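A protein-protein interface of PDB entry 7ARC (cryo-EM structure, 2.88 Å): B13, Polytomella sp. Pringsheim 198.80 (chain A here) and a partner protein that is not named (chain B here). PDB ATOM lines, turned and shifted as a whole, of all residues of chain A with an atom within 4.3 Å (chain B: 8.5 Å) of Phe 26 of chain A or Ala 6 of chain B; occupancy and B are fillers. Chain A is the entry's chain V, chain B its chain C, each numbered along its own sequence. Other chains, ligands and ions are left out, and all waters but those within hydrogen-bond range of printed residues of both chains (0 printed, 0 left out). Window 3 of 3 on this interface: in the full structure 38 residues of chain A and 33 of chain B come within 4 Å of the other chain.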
ATOM      1  N   PHE A  26      25.842  21.300   2.369  1.00  0.00           N
ATOM      2  CA  PHE A  26      25.401  20.211   1.510  1.00  0.00           C
ATOM      3  C   PHE A  26      26.543  19.742   0.619  1.00  0.00           C
ATOM      4  O   PHE A  26      27.598  20.368   0.574  1.00  0.00           O
ATOM      5  CB  PHE A  26      24.196  20.650   0.673  1.00  0.00           C
ATOM      6  CG  PHE A  26      24.513  21.694  -0.364  1.00  0.00           C
ATOM      7  CD1 PHE A  26      24.936  21.332  -1.634  1.00  0.00           C
ATOM      8  CD2 PHE A  26      24.385  23.038  -0.070  1.00  0.00           C
ATOM      9  CE1 PHE A  26      25.225  22.288  -2.582  1.00  0.00           C
ATOM     10  CE2 PHE A  26      24.673  23.998  -1.017  1.00  0.00           C
ATOM     11  CZ  PHE A  26      25.094  23.622  -2.273  1.00  0.00           C
ATOM     12  N   LYS A  27      26.331  18.639  -0.095  1.00  0.00           N
ATOM     13  CA  LYS A  27      27.329  18.093  -1.002  1.00  0.00           C
ATOM     14  C   LYS A  27      26.767  18.008  -2.412  1.00  0.00           C
ATOM     15  O   LYS A  27      25.692  17.439  -2.623  1.00  0.00           O
ATOM     16  CB  LYS A  27      27.796  16.709  -0.549  1.00  0.00           C
ATOM     17  CG  LYS A  27      28.884  16.122  -1.432  1.00  0.00           C
ATOM     18  CD  LYS A  27      29.401  14.807  -0.890  1.00  0.00           C
ATOM     19  CE  LYS A  27      30.378  14.162  -1.860  1.00  0.00           C
ATOM     20  NZ  LYS A  27      31.626  14.955  -2.020  1.00  0.00           N
ATOM     21  N   ALA A  28      27.495  18.578  -3.366  1.00  0.00           N
ATOM     22  CA  ALA A  28      27.123  18.473  -4.767  1.00  0.00           C
ATOM     23  C   ALA A  28      27.338  17.047  -5.258  1.00  0.00           C
ATOM     24  O   ALA A  28      28.325  16.396  -4.907  1.00  0.00           O
ATOM     25  CB  ALA A  28      27.938  19.448  -5.610  1.00  0.00           C
ATOM     26  N   LEU A  42      26.708  28.758  -7.607  1.00  0.00           N
ATOM     27  CA  LEU A  42      25.845  28.163  -6.591  1.00  0.00           C
ATOM     28  C   LEU A  42      24.376  28.259  -6.983  1.00  0.00           C
ATOM     29  O   LEU A  42      23.639  27.269  -6.918  1.00  0.00           O
ATOM     30  CB  LEU A  42      26.084  28.839  -5.242  1.00  0.00           C
ATOM     31  CG  LEU A  42      25.290  28.293  -4.056  1.00  0.00           C
ATOM     32  CD1 LEU A  42      25.644  26.849  -3.777  1.00  0.00           C
ATOM     33  CD2 LEU A  42      25.534  29.147  -2.826  1.00  0.00           C
ATOM     34  N   VAL A  46      21.829  24.984  -7.883  1.00  0.00           N
ATOM     35  CA  VAL A  46      20.677  24.588  -7.074  1.00  0.00           C
ATOM     36  C   VAL A  46      19.353  24.925  -7.734  1.00  0.00           C
ATOM     37  O   VAL A  46      18.297  24.577  -7.191  1.00  0.00           O
ATOM     38  CB  VAL A  46      20.729  25.220  -5.670  1.00  0.00           C
ATOM     39  CG1 VAL A  46      22.016  24.834  -4.966  1.00  0.00           C
ATOM     40  CG2 VAL A  46      20.608  26.721  -5.764  1.00  0.00           C
ATOM     41  N   HIS A 112      17.644  33.163  -0.219  1.00  0.00           N
ATOM     42  CA  HIS A 112      18.089  33.799  -1.448  1.00  0.00           C
ATOM     43  C   HIS A 112      17.248  35.039  -1.734  1.00  0.00           C
ATOM     44  O   HIS A 112      16.071  35.109  -1.375  1.00  0.00           O
ATOM     45  CB  HIS A 112      17.982  32.828  -2.622  1.00  0.00           C
ATOM     46  CG  HIS A 112      19.018  31.749  -2.615  1.00  0.00           C
ATOM     47  ND1 HIS A 112      20.287  31.933  -3.117  1.00  0.00           N
ATOM     48  CD2 HIS A 112      18.968  30.470  -2.175  1.00  0.00           C
ATOM     49  CE1 HIS A 112      20.977  30.815  -2.982  1.00  0.00           C
ATOM     50  NE2 HIS A 112      20.200  29.912  -2.413  1.00  0.00           N
ATOM     51  N   TYR B   3      10.887  28.321   0.087  1.00  0.00           N
ATOM     52  CA  TYR B   3      11.388  27.058  -0.425  1.00  0.00           C
ATOM     53  C   TYR B   3      12.821  26.892   0.060  1.00  0.00           C
ATOM     54  O   TYR B   3      13.660  27.769  -0.167  1.00  0.00           O
ATOM     55  CB  TYR B   3      11.313  27.044  -1.949  1.00  0.00           C
ATOM     56  CG  TYR B   3       9.996  27.574  -2.460  1.00  0.00           C
ATOM     57  CD1 TYR B   3       8.811  26.897  -2.217  1.00  0.00           C
ATOM     58  CD2 TYR B   3       9.934  28.767  -3.162  1.00  0.00           C
ATOM     59  CE1 TYR B   3       7.605  27.384  -2.671  1.00  0.00           C
ATOM     60  CE2 TYR B   3       8.731  29.263  -3.619  1.00  0.00           C
ATOM     61  CZ  TYR B   3       7.572  28.567  -3.372  1.00  0.00           C
ATOM     62  OH  TYR B   3       6.373  29.058  -3.828  1.00  0.00           O
ATOM     63  N   CYS B   4      13.107  25.782   0.735  1.00  0.00           N
ATOM     64  CA  CYS B   4      14.408  25.611   1.377  1.00  0.00           C
ATOM     65  C   CYS B   4      15.460  25.256   0.327  1.00  0.00           C
ATOM     66  O   CYS B   4      16.066  24.186   0.331  1.00  0.00           O
ATOM     67  CB  CYS B   4      14.328  24.554   2.470  1.00  0.00           C
ATOM     68  SG  CYS B   4      13.732  25.175   4.056  1.00  0.00           S
ATOM     69  N   TYR B   5      15.671  26.203  -0.584  1.00  0.00           N
ATOM     70  CA  TYR B   5      16.733  26.085  -1.567  1.00  0.00           C
ATOM     71  C   TYR B   5      18.087  26.099  -0.875  1.00  0.00           C
ATOM     72  O   TYR B   5      18.332  26.907   0.024  1.00  0.00           O
ATOM     73  CB  TYR B   5      16.652  27.240  -2.563  1.00  0.00           C
ATOM     74  CG  TYR B   5      15.876  26.934  -3.821  1.00  0.00           C
ATOM     75  CD1 TYR B   5      16.308  25.964  -4.710  1.00  0.00           C
ATOM     76  CD2 TYR B   5      14.713  27.627  -4.120  1.00  0.00           C
ATOM     77  CE1 TYR B   5      15.599  25.689  -5.860  1.00  0.00           C
ATOM     78  CE2 TYR B   5      14.000  27.359  -5.266  1.00  0.00           C
ATOM     79  CZ  TYR B   5      14.448  26.392  -6.133  1.00  0.00           C
ATOM     80  OH  TYR B   5      13.738  26.122  -7.279  1.00  0.00           O
ATOM     81  N   ALA B   6      18.966  25.190  -1.290  1.00  0.00           N
ATOM     82  CA  ALA B   6      20.265  25.069  -0.647  1.00  0.00           C
ATOM     83  C   ALA B   6      21.048  26.358  -0.832  1.00  0.00           C
ATOM     84  O   ALA B   6      21.330  26.766  -1.962  1.00  0.00           O
ATOM     85  CB  ALA B   6      21.031  23.884  -1.230  1.00  0.00           C
ATOM     86  N   ARG B   7      21.392  27.006   0.277  1.00  0.00           N
ATOM     87  CA  ARG B   7      22.138  28.257   0.233  1.00  0.00           C
ATOM     88  C   ARG B   7      23.519  28.152   0.855  1.00  0.00           C
ATOM     89  O   ARG B   7      24.512  28.506   0.211  1.00  0.00           O
ATOM     90  CB  ARG B   7      21.340  29.359   0.940  1.00  0.00           C
ATOM     91  CG  ARG B   7      21.788  30.762   0.607  1.00  0.00           C
ATOM     92  CD  ARG B   7      20.971  31.769   1.382  1.00  0.00           C
ATOM     93  NE  ARG B   7      20.822  31.360   2.773  1.00  0.00           N
ATOM     94  CZ  ARG B   7      21.629  31.742   3.752  1.00  0.00           C
ATOM     95  NH1 ARG B   7      22.664  32.532   3.524  1.00  0.00           N
ATOM     96  NH2 ARG B   7      21.398  31.312   4.989  1.00  0.00           N
ATOM     97  N   LYS B   8      23.614  27.672   2.089  1.00  0.00           N
ATOM     98  CA  LYS B   8      24.873  27.668   2.819  1.00  0.00           C
ATOM     99  C   LYS B   8      25.612  26.369   2.524  1.00  0.00           C
ATOM    100  O   LYS B   8      25.086  25.278   2.772  1.00  0.00           O
ATOM    101  CB  LYS B   8      24.630  27.853   4.316  1.00  0.00           C
ATOM    102  CG  LYS B   8      25.897  27.994   5.128  1.00  0.00           C
ATOM    103  CD  LYS B   8      25.604  28.126   6.609  1.00  0.00           C
ATOM    104  CE  LYS B   8      25.042  29.504   6.918  1.00  0.00           C
ATOM    105  NZ  LYS B   8      24.848  29.730   8.375  1.00  0.00           N
ATOM    106  N   MET B   9      26.831  26.490   1.998  1.00  0.00           N
ATOM    107  CA  MET B   9      27.605  25.321   1.596  1.00  0.00           C
ATOM    108  C   MET B   9      28.235  24.594   2.777  1.00  0.00           C
ATOM    109  O   MET B   9      28.360  23.365   2.742  1.00  0.00           O
ATOM    110  CB  MET B   9      28.689  25.743   0.604  1.00  0.00           C
ATOM    111  CG  MET B   9      29.534  24.608   0.058  1.00  0.00           C
ATOM    112  SD  MET B   9      28.711  23.687  -1.252  1.00  0.00           S
ATOM    113  CE  MET B   9      29.675  22.177  -1.251  1.00  0.00           C
ATOM    114  N   THR B  10      28.625  25.315   3.824  1.00  0.00           N
ATOM    115  CA  THR B  10      29.256  24.685   4.974  1.00  0.00           C
ATOM    116  C   THR B  10      28.868  25.423   6.245  1.00  0.00           C
ATOM    117  O   THR B  10      28.542  26.611   6.215  1.00  0.00           O
ATOM    118  CB  THR B  10      30.784  24.654   4.829  1.00  0.00           C
ATOM    119  OG1 THR B  10      31.359  23.979   5.953  1.00  0.00           O
ATOM    120  CG2 THR B  10      31.343  26.063   4.743  1.00  0.00           C
ATOM    121  N   ASP B  11      28.878  24.683   7.359  1.00  0.00           N
ATOM    122  CA  ASP B  11      28.576  25.181   8.700  1.00  0.00           C
ATOM    123  C   ASP B  11      27.095  25.466   8.912  1.00  0.00           C
ATOM    124  O   ASP B  11      26.735  26.218   9.823  1.00  0.00           O
ATOM    125  CB  ASP B  11      29.400  26.427   9.055  1.00  0.00           C
ATOM    126  CG  ASP B  11      30.854  26.300   8.647  1.00  0.00           C
ATOM    127  OD1 ASP B  11      31.512  25.334   9.087  1.00  0.00           O
ATOM    128  OD2 ASP B  11      31.339  27.166   7.888  1.00  0.00           O
ATOM    129  N   LYS B  12      26.217  24.886   8.093  1.00  0.00           N
ATOM    130  CA  LYS B  12      24.788  24.962   8.369  1.00  0.00           C
ATOM    131  C   LYS B  12      24.405  23.874   9.368  1.00  0.00           C
ATOM    132  O   LYS B  12      23.516  23.057   9.111  1.00  0.00           O
ATOM    133  CB  LYS B  12      23.989  24.842   7.067  1.00  0.00           C
ATOM    134  CG  LYS B  12      22.482  25.035   7.197  1.00  0.00           C
ATOM    135  CD  LYS B  12      21.807  24.978   5.838  1.00  0.00           C
ATOM    136  CE  LYS B  12      20.307  25.162   5.957  1.00  0.00           C
ATOM    137  NZ  LYS B  12      19.644  25.104   4.626  1.00  0.00           N
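Among the printed residues, pairs that only touch across the chains: Phe 26 of chain A with Ala 6 of chain B (3.6 Å), Phe 26 of chain A with Lys 8 of chain B (3.7 Å), Leu 42 of chain A with Arg 7 of chain B (3.3 Å), Val 46 of chain A with Tyr 5 of chain B (3.2 Å), Val 46 of chain A with Ala 6 of chain B (3.6 Å), His 112 of chain A with Tyr 5 of chain B (3.99 Å) and His 112 of chain A with Arg 7 of chain B (3.5 Å).
Of the 6 printed residues of chain A, 4 touch a printed residue of chain B. Hydrophobic or aromatic side chains of chain A that line the printed part of chain B: Phe 26, Leu 42, Val 46 and His 112. Of the 10 printed residues of chain B, 5 touch a printed residue of chain A. Along chain B the printed residues that touch a printed residue of chain A span positions 5 to 9. Among the printed residues, no Asp or Glu carboxylate lies within 4 Å of a Lys or Arg side-chain nitrogen of the other chain.
The backbone NH (N) of Phe 26 of chain A lies within hydrogen-bond range of the backbone carbonyl oxygen (O) of Met 9 of chain B, at 3.3 Å. NE2 of His 112 of chain A lies within hydrogen-bond range of O of Ala 6 of chain B (3.4 Å).
Of chain B, only Ala 6 (3.6 Å), Lys 8 (3.7 Å) and Met 9 (3.3 Å) come within 4 Å of Phe 26 of chain A. Lys 27 of chain A touches none of the printed residues of chain B. Of the printed residues of chain B, Leu 42 of chain A touches Arg 7. Of the printed residues of chain B, Val 46 of chain A touches Tyr 5 and Ala 6. Tyr 3 of chain B touches none of the printed residues of chain A. Of the printed residues of chain A, Tyr 5 of chain B touches Val 46 (3.2 Å) and His 112 (3.99 Å). Ala 6 of chain B touches just these residues of chain A: Phe 26 (3.6 Å), Val 46 (3.6 Å) and His 112 (3.4 Å). Of the printed residues of chain A, Met 9 of chain B touches Phe 26. The nearest residue of chain B that does not touch Phe 26 of chain A is Arg 7 of chain B (4.6 Å).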
